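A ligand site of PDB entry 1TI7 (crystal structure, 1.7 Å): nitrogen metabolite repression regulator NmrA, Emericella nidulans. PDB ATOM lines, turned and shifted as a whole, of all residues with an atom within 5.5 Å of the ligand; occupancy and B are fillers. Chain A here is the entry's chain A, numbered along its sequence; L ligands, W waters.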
ATOM      1  N   ASN A  12       1.413  -8.727   6.742  1.00  0.00           N
ATOM      2  CA  ASN A  12      -0.012  -9.054   6.586  1.00  0.00           C
ATOM      3  C   ASN A  12      -0.811  -8.154   7.523  1.00  0.00           C
ATOM      4  O   ASN A  12      -1.701  -8.599   8.252  1.00  0.00           O
ATOM      5  CB  ASN A  12      -0.255 -10.532   6.888  1.00  0.00           C
ATOM      6  CG  ASN A  12       0.279 -11.425   5.787  1.00  0.00           C
ATOM      7  OD1 ASN A  12      -0.036 -11.228   4.609  1.00  0.00           O
ATOM      8  ND2 ASN A  12       1.085 -12.414   6.157  1.00  0.00           N
ATOM      9  N   THR A  14      -3.250  -6.093   7.234  1.00  0.00           N
ATOM     10  CA  THR A  14      -4.712  -5.964   7.182  1.00  0.00           C
ATOM     11  C   THR A  14      -5.422  -7.209   7.708  1.00  0.00           C
ATOM     12  O   THR A  14      -6.636  -7.268   7.761  1.00  0.00           O
ATOM     13  CB  THR A  14      -5.222  -5.658   5.737  1.00  0.00           C
ATOM     14  OG1 THR A  14      -4.875  -6.721   4.855  1.00  0.00           O
ATOM     15  CG2 THR A  14      -4.599  -4.351   5.206  1.00  0.00           C
ATOM     16  N   GLY A  15      -4.636  -8.207   8.128  1.00  0.00           N
ATOM     17  CA  GLY A  15      -5.216  -9.416   8.689  1.00  0.00           C
ATOM     18  C   GLY A  15      -5.645  -9.137  10.117  1.00  0.00           C
ATOM     19  O   GLY A  15      -5.093  -8.267  10.785  1.00  0.00           O
ATOM     20  N   ARG A  16      -6.626  -9.894  10.606  1.00  0.00           N
ATOM     21  CA  ARG A  16      -7.150  -9.673  11.950  1.00  0.00           C
ATOM     22  C   ARG A  16      -6.127  -9.677  13.081  1.00  0.00           C
ATOM     23  O   ARG A  16      -6.203  -8.830  13.980  1.00  0.00           O
ATOM     24  CB  ARG A  16      -8.271 -10.681  12.230  1.00  0.00           C
ATOM     25  CG  ARG A  16      -9.610 -10.249  11.635  1.00  0.00           C
ATOM     26  CD  ARG A  16     -10.597 -11.408  11.583  1.00  0.00           C
ATOM     27  NE  ARG A  16     -10.240 -12.332  10.520  1.00  0.00           N
ATOM     28  CZ  ARG A  16     -11.007 -13.333  10.109  1.00  0.00           C
ATOM     29  NH1 ARG A  16     -12.175 -13.552  10.701  1.00  0.00           N
ATOM     30  NH2 ARG A  16     -10.618 -14.093   9.101  1.00  0.00           N
ATOM     31  N   GLN A  17      -5.166 -10.600  13.056  1.00  0.00           N
ATOM     32  CA  GLN A  17      -4.184 -10.637  14.125  1.00  0.00           C
ATOM     33  C   GLN A  17      -3.294  -9.389  14.131  1.00  0.00           C
ATOM     34  O   GLN A  17      -3.170  -8.722  15.152  1.00  0.00           O
ATOM     35  CB  GLN A  17      -3.283 -11.878  13.998  1.00  0.00           C
ATOM     36  CG  GLN A  17      -3.999 -13.200  14.287  1.00  0.00           C
ATOM     37  CD  GLN A  17      -3.083 -14.398  14.132  1.00  0.00           C
ATOM     38  OE1 GLN A  17      -1.905 -14.324  14.480  1.00  0.00           O
ATOM     39  NE2 GLN A  17      -3.614 -15.507  13.630  1.00  0.00           N
ATOM     40  N   ALA A  18      -2.677  -9.094  12.996  1.00  0.00           N
ATOM     41  CA  ALA A  18      -1.776  -7.945  12.923  1.00  0.00           C
ATOM     42  C   ALA A  18      -2.523  -6.635  13.136  1.00  0.00           C
ATOM     43  O   ALA A  18      -2.035  -5.751  13.845  1.00  0.00           O
ATOM     44  CB  ALA A  18      -1.052  -7.930  11.553  1.00  0.00           C
ATOM     45  N   HIS A  37      -0.108  -6.379   1.332  1.00  0.00           N
ATOM     46  CA  HIS A  37       0.061  -6.825  -0.042  1.00  0.00           C
ATOM     47  C   HIS A  37      -0.372  -5.705  -1.001  1.00  0.00           C
ATOM     48  O   HIS A  37       0.154  -5.611  -2.115  1.00  0.00           O
ATOM     49  CB  HIS A  37      -0.667  -8.163  -0.264  1.00  0.00           C
ATOM     50  CG  HIS A  37      -2.077  -8.032  -0.764  1.00  0.00           C
ATOM     51  ND1 HIS A  37      -2.383  -7.819  -2.088  1.00  0.00           N
ATOM     52  CD2 HIS A  37      -3.263  -8.166  -0.120  1.00  0.00           C
ATOM     53  CE1 HIS A  37      -3.696  -7.831  -2.237  1.00  0.00           C
ATOM     54  NE2 HIS A  37      -4.253  -8.040  -1.060  1.00  0.00           N
ATOM     55  N   SER A  38      -1.288  -4.848  -0.560  1.00  0.00           N
ATOM     56  CA  SER A  38      -1.748  -3.702  -1.352  1.00  0.00           C
ATOM     57  C   SER A  38      -2.344  -2.624  -0.439  1.00  0.00           C
ATOM     58  O   SER A  38      -2.886  -2.934   0.618  1.00  0.00           O
ATOM     59  CB  SER A  38      -2.782  -4.131  -2.406  1.00  0.00           C
ATOM     60  OG  SER A  38      -4.006  -4.514  -1.816  1.00  0.00           O
ATOM     61  N   LYS A  40      -4.958  -0.670  -0.922  1.00  0.00           N
ATOM     62  CA  LYS A  40      -6.398  -0.447  -1.003  1.00  0.00           C
ATOM     63  C   LYS A  40      -7.165  -1.247   0.046  1.00  0.00           C
ATOM     64  O   LYS A  40      -6.614  -2.151   0.684  1.00  0.00           O
ATOM     65  CB  LYS A  40      -6.895  -0.813  -2.394  1.00  0.00           C
ATOM     66  CG  LYS A  40      -6.594  -2.243  -2.805  1.00  0.00           C
ATOM     67  CD  LYS A  40      -7.214  -2.571  -4.159  1.00  0.00           C
ATOM     68  CE  LYS A  40      -6.868  -3.990  -4.604  1.00  0.00           C
ATOM     69  NZ  LYS A  40      -7.325  -5.016  -3.634  1.00  0.00           N
ATOM     70  N   GLY A  41      -8.445  -0.917   0.219  1.00  0.00           N
ATOM     71  CA  GLY A  41      -9.250  -1.646   1.187  1.00  0.00           C
ATOM     72  C   GLY A  41      -9.476  -0.851   2.453  1.00  0.00           C
ATOM     73  O   GLY A  41      -8.647  -0.021   2.830  1.00  0.00           O
ATOM     74  N   ASN A  80       2.884 -12.956  11.277  1.00  0.00           N
ATOM     75  CA  ASN A  80       1.812 -13.914  11.034  1.00  0.00           C
ATOM     76  C   ASN A  80       1.648 -13.984   9.532  1.00  0.00           C
ATOM     77  O   ASN A  80       1.165 -13.037   8.911  1.00  0.00           O
ATOM     78  CB  ASN A  80       0.495 -13.445  11.669  1.00  0.00           C
ATOM     79  CG  ASN A  80      -0.675 -14.371  11.350  1.00  0.00           C
ATOM     80  OD1 ASN A  80      -0.573 -15.595  11.492  1.00  0.00           O
ATOM     81  ND2 ASN A  80      -1.804 -13.786  10.908  1.00  0.00           N
ATOM     82  N   THR A  81       2.068 -15.095   8.931  1.00  0.00           N
ATOM     83  CA  THR A  81       1.935 -15.263   7.486  1.00  0.00           C
ATOM     84  C   THR A  81       0.585 -15.884   7.146  1.00  0.00           C
ATOM     85  O   THR A  81      -0.189 -16.255   8.037  1.00  0.00           O
ATOM     86  CB  THR A  81       3.063 -16.163   6.946  1.00  0.00           C
ATOM     87  OG1 THR A  81       3.130 -17.368   7.725  1.00  0.00           O
ATOM     88  CG2 THR A  81       4.406 -15.438   7.043  1.00  0.00           C
ATOM     89  N   THR A  82       0.293 -15.973   5.843  1.00  0.00           N
ATOM     90  CA  THR A  82      -0.953 -16.576   5.359  1.00  0.00           C
ATOM     91  C   THR A  82      -0.614 -17.340   4.099  1.00  0.00           C
ATOM     92  O   THR A  82       0.389 -17.061   3.440  1.00  0.00           O
ATOM     93  CB  THR A  82      -2.004 -15.521   4.989  1.00  0.00           C
ATOM     94  OG1 THR A  82      -1.534 -14.744   3.886  1.00  0.00           O
ATOM     95  CG2 THR A  82      -2.287 -14.620   6.162  1.00  0.00           C
ATOM     96  N   SER A  83      -1.444 -18.324   3.746  1.00  0.00           N
ATOM     97  CA  SER A  83      -1.192 -19.120   2.550  1.00  0.00           C
ATOM     98  C   SER A  83      -1.503 -18.333   1.284  1.00  0.00           C
ATOM     99  O   SER A  83      -1.048 -18.694   0.194  1.00  0.00           O
ATOM    100  CB  SER A  83      -2.022 -20.412   2.588  1.00  0.00           C
ATOM    101  OG  SER A  83      -3.409 -20.128   2.693  1.00  0.00           O
ATOM    102  N   GLN A  84      -2.267 -17.257   1.426  1.00  0.00           N
ATOM    103  CA  GLN A  84      -2.632 -16.400   0.288  1.00  0.00           C
ATOM    104  C   GLN A  84      -1.411 -15.741  -0.336  1.00  0.00           C
ATOM    105  O   GLN A  84      -1.388 -15.499  -1.542  1.00  0.00           O
ATOM    106  CB  GLN A  84      -3.619 -15.327   0.736  1.00  0.00           C
ATOM    107  CG  GLN A  84      -4.950 -15.867   1.218  1.00  0.00           C
ATOM    108  CD  GLN A  84      -5.375 -15.240   2.519  1.00  0.00           C
ATOM    109  OE1 GLN A  84      -4.684 -15.332   3.528  1.00  0.00           O
ATOM    110  NE2 GLN A  84      -6.543 -14.588   2.513  1.00  0.00           N
ATOM    111  N   ALA A  85      -0.404 -15.459   0.487  1.00  0.00           N
ATOM    112  CA  ALA A  85       0.822 -14.831   0.006  1.00  0.00           C
ATOM    113  C   ALA A  85       1.710 -15.823  -0.741  1.00  0.00           C
ATOM    114  O   ALA A  85       2.642 -15.424  -1.437  1.00  0.00           O
ATOM    115  CB  ALA A  85       1.600 -14.230   1.172  1.00  0.00           C
ATOM    116  N   GLU A  88       4.375 -20.285   2.232  1.00  0.00           N
ATOM    117  CA  GLU A  88       4.454 -19.860   3.613  1.00  0.00           C
ATOM    118  C   GLU A  88       5.763 -20.227   4.319  1.00  0.00           C
ATOM    119  O   GLU A  88       6.283 -19.447   5.122  1.00  0.00           O
ATOM    120  CB  GLU A  88       3.269 -20.444   4.355  1.00  0.00           C
ATOM    121  CG  GLU A  88       3.078 -19.951   5.736  1.00  0.00           C
ATOM    122  CD  GLU A  88       1.602 -19.877   6.101  1.00  0.00           C
ATOM    123  OE1 GLU A  88       0.786 -20.629   5.527  1.00  0.00           O
ATOM    124  OE2 GLU A  88       1.265 -19.083   6.986  1.00  0.00           O
ATOM    125  N   MET A 113       1.121 -22.701  14.410  1.00  0.00           N
ATOM    126  CA  MET A 113      -0.024 -23.588  14.545  1.00  0.00           C
ATOM    127  C   MET A 113       0.543 -24.994  14.622  1.00  0.00           C
ATOM    128  O   MET A 113       1.709 -25.210  14.314  1.00  0.00           O
ATOM    129  CB  MET A 113      -1.004 -23.420  13.380  1.00  0.00           C
ATOM    130  CG  MET A 113      -1.879 -22.143  13.481  1.00  0.00           C
ATOM    131  SD  MET A 113      -2.915 -22.086  14.953  1.00  0.00           S
ATOM    132  CE  MET A 113      -4.357 -23.039  14.414  1.00  0.00           C
ATOM    133  N   MET A 127      -3.007 -25.801   6.332  1.00  0.00           N
ATOM    134  CA  MET A 127      -2.716 -24.373   6.514  1.00  0.00           C
ATOM    135  C   MET A 127      -2.117 -24.126   7.893  1.00  0.00           C
ATOM    136  O   MET A 127      -1.783 -22.983   8.234  1.00  0.00           O
ATOM    137  CB  MET A 127      -3.987 -23.545   6.329  1.00  0.00           C
ATOM    138  CG  MET A 127      -4.597 -23.718   4.957  1.00  0.00           C
ATOM    139  SD  MET A 127      -6.089 -22.746   4.706  1.00  0.00           S
ATOM    140  CE  MET A 127      -5.991 -22.476   2.921  1.00  0.00           C
ATOM    141  N   TRP A 128      -1.953 -25.184   8.670  1.00  0.00           N
ATOM    142  CA  TRP A 128      -1.391 -25.052  10.012  1.00  0.00           C
ATOM    143  C   TRP A 128       0.014 -25.623  10.121  1.00  0.00           C
ATOM    144  O   TRP A 128       0.928 -24.949  10.572  1.00  0.00           O
ATOM    145  CB  TRP A 128      -2.269 -25.735  11.067  1.00  0.00           C
ATOM    146  CG  TRP A 128      -3.669 -25.179  11.211  1.00  0.00           C
ATOM    147  CD1 TRP A 128      -4.147 -24.010  10.699  1.00  0.00           C
ATOM    148  CD2 TRP A 128      -4.759 -25.795  11.903  1.00  0.00           C
ATOM    149  NE1 TRP A 128      -5.484 -23.860  11.022  1.00  0.00           N
ATOM    150  CE2 TRP A 128      -5.885 -24.946  11.750  1.00  0.00           C
ATOM    151  CE3 TRP A 128      -4.906 -27.000  12.625  1.00  0.00           C
ATOM    152  CZ2 TRP A 128      -7.141 -25.256  12.306  1.00  0.00           C
ATOM    153  CZ3 TRP A 128      -6.150 -27.303  13.179  1.00  0.00           C
ATOM    154  CH2 TRP A 128      -7.254 -26.438  13.010  1.00  0.00           C
ATOM    155  N   LYS A 131       3.325 -23.718   9.369  1.00  0.00           N
ATOM    156  CA  LYS A 131       3.769 -22.714  10.331  1.00  0.00           C
ATOM    157  C   LYS A 131       4.662 -23.347  11.380  1.00  0.00           C
ATOM    158  O   LYS A 131       5.606 -22.725  11.866  1.00  0.00           O
ATOM    159  CB  LYS A 131       2.567 -22.054  11.036  1.00  0.00           C
ATOM    160  CG  LYS A 131       1.593 -21.328  10.117  1.00  0.00           C
ATOM    161  CD  LYS A 131       0.491 -20.699  10.967  1.00  0.00           C
ATOM    162  CE  LYS A 131      -0.622 -20.055  10.125  1.00  0.00           C
ATOM    163  NZ  LYS A 131      -0.099 -18.979   9.230  1.00  0.00           N
ATOM    164  N   ALA A 150      -3.021 -19.220  17.806  1.00  0.00           N
ATOM    165  CA  ALA A 150      -4.365 -18.645  17.860  1.00  0.00           C
ATOM    166  C   ALA A 150      -5.496 -19.667  17.919  1.00  0.00           C
ATOM    167  O   ALA A 150      -5.528 -20.630  17.145  1.00  0.00           O
ATOM    168  CB  ALA A 150      -4.577 -17.736  16.645  1.00  0.00           C
ATOM    169  N   GLY A 151      -6.422 -19.431  18.847  1.00  0.00           N
ATOM    170  CA  GLY A 151      -7.581 -20.292  18.964  1.00  0.00           C
ATOM    171  C   GLY A 151      -8.525 -19.945  17.829  1.00  0.00           C
ATOM    172  O   GLY A 151      -8.219 -19.073  17.000  1.00  0.00           O
ATOM    173  N   ILE A 152      -9.683 -20.601  17.768  1.00  0.00           N
ATOM    174  CA  ILE A 152     -10.637 -20.326  16.697  1.00  0.00           C
ATOM    175  C   ILE A 152     -11.274 -18.953  16.896  1.00  0.00           C
ATOM    176  O   ILE A 152     -11.711 -18.626  17.999  1.00  0.00           O
ATOM    177  CB  ILE A 152     -11.748 -21.393  16.693  1.00  0.00           C
ATOM    178  CG1 ILE A 152     -11.122 -22.792  16.660  1.00  0.00           C
ATOM    179  CG2 ILE A 152     -12.653 -21.192  15.501  1.00  0.00           C
ATOM    180  CD1 ILE A 152     -12.157 -23.900  16.876  1.00  0.00           C
ATOM    181  N   TYR A 153     -11.334 -18.150  15.830  1.00  0.00           N
ATOM    182  CA  TYR A 153     -11.885 -16.807  15.921  1.00  0.00           C
ATOM    183  C   TYR A 153     -13.387 -16.758  16.144  1.00  0.00           C
ATOM    184  O   TYR A 153     -14.145 -17.398  15.412  1.00  0.00           O
ATOM    185  CB  TYR A 153     -11.638 -15.996  14.658  1.00  0.00           C
ATOM    186  CG  TYR A 153     -10.213 -15.684  14.284  1.00  0.00           C
ATOM    187  CD1 TYR A 153      -9.127 -16.208  15.005  1.00  0.00           C
ATOM    188  CD2 TYR A 153      -9.940 -14.956  13.140  1.00  0.00           C
ATOM    189  CE1 TYR A 153      -7.805 -16.000  14.564  1.00  0.00           C
ATOM    190  CE2 TYR A 153      -8.646 -14.741  12.687  1.00  0.00           C
ATOM    191  CZ  TYR A 153      -7.589 -15.259  13.395  1.00  0.00           C
ATOM    192  OH  TYR A 153      -6.328 -15.077  12.885  1.00  0.00           O
ATOM    193  N   ASN A 156     -15.290 -15.739  13.045  1.00  0.00           N
ATOM    194  CA  ASN A 156     -15.309 -16.552  11.828  1.00  0.00           C
ATOM    195  C   ASN A 156     -16.812 -16.711  11.529  1.00  0.00           C
ATOM    196  O   ASN A 156     -17.212 -16.936  10.393  1.00  0.00           O
ATOM    197  CB  ASN A 156     -14.798 -17.979  12.049  1.00  0.00           C
ATOM    198  CG  ASN A 156     -13.290 -18.069  12.061  1.00  0.00           C
ATOM    199  OD1 ASN A 156     -12.603 -17.269  11.430  1.00  0.00           O
ATOM    200  ND2 ASN A 156     -12.764 -19.078  12.771  1.00  0.00           N
ATOM    201  N   PHE A 165     -18.055 -22.339   9.640  1.00  0.00           N
ATOM    202  CA  PHE A 165     -18.556 -21.481  10.695  1.00  0.00           C
ATOM    203  C   PHE A 165     -19.775 -20.665  10.285  1.00  0.00           C
ATOM    204  O   PHE A 165     -19.837 -19.460  10.508  1.00  0.00           O
ATOM    205  CB  PHE A 165     -17.440 -20.555  11.187  1.00  0.00           C
ATOM    206  CG  PHE A 165     -16.270 -21.309  11.791  1.00  0.00           C
ATOM    207  CD1 PHE A 165     -16.377 -21.922  13.033  1.00  0.00           C
ATOM    208  CD2 PHE A 165     -15.089 -21.470  11.067  1.00  0.00           C
ATOM    209  CE1 PHE A 165     -15.332 -22.687  13.556  1.00  0.00           C
ATOM    210  CE2 PHE A 165     -14.028 -22.237  11.583  1.00  0.00           C
ATOM    211  CZ  PHE A 165     -14.147 -22.843  12.824  1.00  0.00           C
ATOM    212  N   GLN A 261      -7.876 -28.028   3.255  1.00  0.00           N
ATOM    213  CA  GLN A 261      -7.846 -27.673   4.666  1.00  0.00           C
ATOM    214  C   GLN A 261      -9.089 -28.252   5.350  1.00  0.00           C
ATOM    215  O   GLN A 261      -9.021 -28.860   6.412  1.00  0.00           O
ATOM    216  CB  GLN A 261      -7.848 -26.152   4.826  1.00  0.00           C
ATOM    217  CG  GLN A 261      -8.035 -25.683   6.261  1.00  0.00           C
ATOM    218  CD  GLN A 261      -6.769 -25.758   7.085  1.00  0.00           C
ATOM    219  OE1 GLN A 261      -5.766 -26.345   6.672  1.00  0.00           O
ATOM    220  NE2 GLN A 261      -6.806 -25.154   8.269  1.00  0.00           N
ATOM    221  N   TYR A 276      -7.621 -29.540  19.310  1.00  0.00           N
ATOM    222  CA  TYR A 276      -7.299 -28.450  18.389  1.00  0.00           C
ATOM    223  C   TYR A 276      -5.820 -28.124  18.591  1.00  0.00           C
ATOM    224  O   TYR A 276      -5.084 -27.890  17.632  1.00  0.00           O
ATOM    225  CB  TYR A 276      -8.206 -27.250  18.716  1.00  0.00           C
ATOM    226  CG  TYR A 276      -7.972 -26.028  17.839  1.00  0.00           C
ATOM    227  CD1 TYR A 276      -7.055 -25.049  18.225  1.00  0.00           C
ATOM    228  CD2 TYR A 276      -8.682 -25.850  16.662  1.00  0.00           C
ATOM    229  CE1 TYR A 276      -6.868 -23.895  17.449  1.00  0.00           C
ATOM    230  CE2 TYR A 276      -8.496 -24.715  15.872  1.00  0.00           C
ATOM    231  CZ  TYR A 276      -7.592 -23.738  16.278  1.00  0.00           C
ATOM    232  OH  TYR A 276      -7.442 -22.595  15.541  1.00  0.00           O
HETATM  233  P1  LIG L   1      -7.269 -12.600   7.963  1.00  0.00           P
HETATM  234  O1  LIG L   1      -7.948 -13.868   7.711  1.00  0.00           O
HETATM  235  O2  LIG L   1      -7.973 -11.659   8.822  1.00  0.00           O
HETATM  236  O3  LIG L   1      -7.076 -11.773   6.598  1.00  0.00           O
HETATM  237  C1  LIG L   1      -6.413 -12.379   5.479  1.00  0.00           C
HETATM  238  C2  LIG L   1      -5.501 -11.339   4.690  1.00  0.00           C
HETATM  239  O4  LIG L   1      -4.675 -11.586   3.531  1.00  0.00           O
HETATM  240  C3  LIG L   1      -6.270 -10.064   4.372  1.00  0.00           C
HETATM  241  O5  LIG L   1      -5.739  -8.974   5.133  1.00  0.00           O
HETATM  242  C4  LIG L   1      -6.112  -9.844   2.887  1.00  0.00           C
HETATM  243  O6  LIG L   1      -5.989  -8.441   2.541  1.00  0.00           O
HETATM  244  C5  LIG L   1      -4.827 -10.542   2.573  1.00  0.00           C
HETATM  245  N1  LIG L   1      -4.696 -11.127   1.185  1.00  0.00           N
HETATM  246  C6  LIG L   1      -5.674 -11.487   0.255  1.00  0.00           C
HETATM  247  N2  LIG L   1      -5.173 -11.964  -0.852  1.00  0.00           N
HETATM  248  C7  LIG L   1      -3.812 -11.925  -0.668  1.00  0.00           C
HETATM  249  C8  LIG L   1      -2.713 -12.294  -1.496  1.00  0.00           C
HETATM  250  N3  LIG L   1      -2.895 -12.783  -2.710  1.00  0.00           N
HETATM  251  N4  LIG L   1      -1.447 -12.126  -1.001  1.00  0.00           N
HETATM  252  C9  LIG L   1      -1.246 -11.617   0.238  1.00  0.00           C
HETATM  253  N5  LIG L   1      -2.222 -11.239   1.077  1.00  0.00           N
HETATM  254  C10 LIG L   1      -3.494 -11.420   0.555  1.00  0.00           C
HETATM  255  O7  LIG L   1      -5.760 -12.787   8.466  1.00  0.00           O
HETATM  256  P2  LIG L   1      -5.312 -13.348   9.894  1.00  0.00           P
HETATM  257  O8  LIG L   1      -6.500 -13.941  10.531  1.00  0.00           O
HETATM  258  O9  LIG L   1      -4.717 -12.287  10.671  1.00  0.00           O
HETATM  259  O10 LIG L   1      -4.230 -14.465   9.471  1.00  0.00           O
HETATM  260  C11 LIG L   1      -4.525 -15.572   8.699  1.00  0.00           C
HETATM  261  C12 LIG L   1      -3.828 -16.775   9.247  1.00  0.00           C
HETATM  262  O11 LIG L   1      -4.458 -17.024  10.543  1.00  0.00           O
HETATM  263  C13 LIG L   1      -4.044 -18.058   8.489  1.00  0.00           C
HETATM  264  O12 LIG L   1      -2.737 -18.541   8.166  1.00  0.00           O
HETATM  265  C14 LIG L   1      -4.849 -19.025   9.435  1.00  0.00           C
HETATM  266  O13 LIG L   1      -4.444 -20.375   9.239  1.00  0.00           O
HETATM  267  C15 LIG L   1      -4.458 -18.443  10.757  1.00  0.00           C
HETATM  268  N6  LIG L   1      -5.442 -18.809  11.802  1.00  0.00           N
HETATM  269  C16 LIG L   1      -6.873 -18.566  11.687  1.00  0.00           C
HETATM  270  C17 LIG L   1      -7.744 -18.964  12.748  1.00  0.00           C
HETATM  271  C18 LIG L   1      -9.229 -18.727  12.624  1.00  0.00           C
HETATM  272  O14 LIG L   1     -10.032 -19.272  13.289  1.00  0.00           O
HETATM  273  N7  LIG L   1      -9.610 -17.812  11.669  1.00  0.00           N
HETATM  274  C19 LIG L   1      -7.192 -19.605  13.918  1.00  0.00           C
HETATM  275  C20 LIG L   1      -5.795 -19.861  14.032  1.00  0.00           C
HETATM  276  C21 LIG L   1      -4.887 -19.469  12.989  1.00  0.00           C
HETATM  277  P3  LIG L   1      -7.121  -7.604   1.774  1.00  0.00           P
HETATM  278  O15 LIG L   1      -8.454  -8.292   1.875  1.00  0.00           O
HETATM  279  O16 LIG L   1      -6.975  -6.329   2.513  1.00  0.00           O
HETATM  280  O17 LIG L   1      -6.577  -7.525   0.414  1.00  0.00           O
HETATM  281  O   HOH W   1       2.063 -10.623   0.698  1.00  0.00           O
HETATM  282  O   HOH W   2       0.969 -10.610  -2.382  1.00  0.00           O
HETATM  283  O   HOH W   3      -5.293  -4.360   0.633  1.00  0.00           O
HETATM  284  O   HOH W   4      -7.327 -21.501  10.328  1.00  0.00           O
HETATM  285  O   HOH W   5      -1.344 -12.348  -5.370  1.00  0.00           O
HETATM  286  O   HOH W   6      -2.354 -10.714  10.464  1.00  0.00           O
HETATM  287  O   HOH W   7      -4.072 -19.229   5.351  1.00  0.00           O
HETATM  288  O   HOH W   8     -11.731  -8.910   1.571  1.00  0.00           O
HETATM  289  O   HOH W   9      -1.952 -17.926  12.643  1.00  0.00           O
HETATM  290  O   HOH W  10      -9.370 -22.020  13.186  1.00  0.00           O
HETATM  291  O   HOH W  11      -7.349 -15.753   5.858  1.00  0.00           O
HETATM  292  O   HOH W  12      -5.228 -11.980  -4.972  1.00  0.00           O
HETATM  293  O   HOH W  13      -6.730 -21.157   7.399  1.00  0.00           O
HETATM  294  O   HOH W  14      -1.927 -20.790   6.774  1.00  0.00           O
HETATM  295  O   HOH W  15      -9.029  -9.559   6.937  1.00  0.00           O
HETATM  296  O   HOH W  16      -8.030 -16.315   9.552  1.00  0.00           O
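Water W6 lies within hydrogen-bond range of O9 of the ligand (2.8 Å), N of Ala 18 (3.0 Å), O of Asn 12 (3.1 Å) and ND2 of Asn 80 (3.2 Å).
Water W15 lies within hydrogen-bond range of an oxygen (O3) of the ligand (3.0 Å) and the backbone carbonyl oxygen of Thr 14 (3.4 Å).
Water W13 bridges O13 of the ligand and SD of Met 127.
Water W7 lies within hydrogen-bond range of the side-chain hydroxyl of Ser 83 (2.9 Å) and an oxygen (O12) of the ligand (3.2 Å).
Water W3 lies within hydrogen-bond range of O of Lys 40, OG of Ser 38 and O16 of the ligand.
Water W4 bridges NE1 of Trp 128 (3.1 Å) and O13 of the ligand (3.3 Å).
The side-chain amide nitrogen (NE2) of Gln 17 sits at hydrogen-bond distance from the side-chain hydroxyl (OH) of Tyr 153, at 2.8 Å.
The side-chain amino group (NZ) of Lys 131 is in hydrogen-bond range of the backbone carbonyl oxygen (O) of Thr 81, 3.0 Å away.
The side-chain amino group (NZ) of Lys 131 is in salt-bridge range of the side-chain carboxylate (OE2) of Glu 88, at 2.6 Å.
The side-chain amide nitrogen of Asn 12 lies within hydrogen-bond range of the backbone carbonyl oxygen of Asn 80 (2.8 Å).
The backbone carbonyl oxygen of Ala 150 is in hydrogen-bond range of the side-chain hydroxyl of Tyr 276, at 3.2 Å.
The side-chain amide oxygen of Gln 84 lies close to the side-chain hydroxyl of Thr 82 (3.2 Å).
The side-chain amide oxygen (OE1) of Gln 261 sits at hydrogen-bond distance from the backbone NH (N) of Met 127 (2.8 Å).
The indole nitrogen (NE1) of Trp 128 lies close to the side-chain amide nitrogen (NE2) of Gln 261 (3.3 Å).
The backbone carbonyl oxygen of Thr 14 lies close to an oxygen (O5) of the ligand (3.3 Å).
The side-chain hydroxyl of Thr 14 sits at hydrogen-bond distance from an oxygen (O5) of the ligand.
An oxygen (O14) of the ligand is in hydrogen-bond range of the backbone NH of Tyr 153, at 3.1 Å.
An oxygen (O8) of the ligand lies within hydrogen-bond range of the side-chain hydroxyl of Tyr 153 (2.6 Å).
The side-chain amide nitrogen (ND2) of Asn 156 lies within hydrogen-bond range of an oxygen (O14) of the ligand, at 2.8 Å.
NE2 of His 37 lies within hydrogen-bond range of O17 of the ligand (2.8 Å).
The backbone NH (N) of Arg 16 sits at hydrogen-bond distance from an oxygen (O2) of the ligand, at 2.8 Å.
An oxygen (O2) of the ligand is in salt-bridge range of the guanidinium group (NE) of Arg 16 (2.9 Å).
O12 of the ligand lies within hydrogen-bond range of NZ of Lys 131 (2.9 Å).
ND2 of Asn 80 is in hydrogen-bond range of O10 of the ligand (2.9 Å).
An oxygen (O9) of the ligand lies within hydrogen-bond range of the backbone NH (N) of Gln 17.
N of Gly 15 is in hydrogen-bond range of O5 of the ligand, 3.3 Å away.
N3 of the ligand is in hydrogen-bond range of O of Gln 84.
O of Thr 81 sits at hydrogen-bond distance from O12 of the ligand (3.4 Å).
Merely in contact with the ligand: Ala 150 (3.2 Å), Gly 151 (3.3 Å), Tyr 276 (3.4 Å), Met 113 (3.5 Å), Thr 82 (3.5 Å), Ile 152 (3.6 Å), Ala 85 (3.7 Å), Met 127 (3.9 Å) and Trp 128 (3.9 Å).
The nearest printed residue that does not touch the ligand is Asn 12 (4.2 Å).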
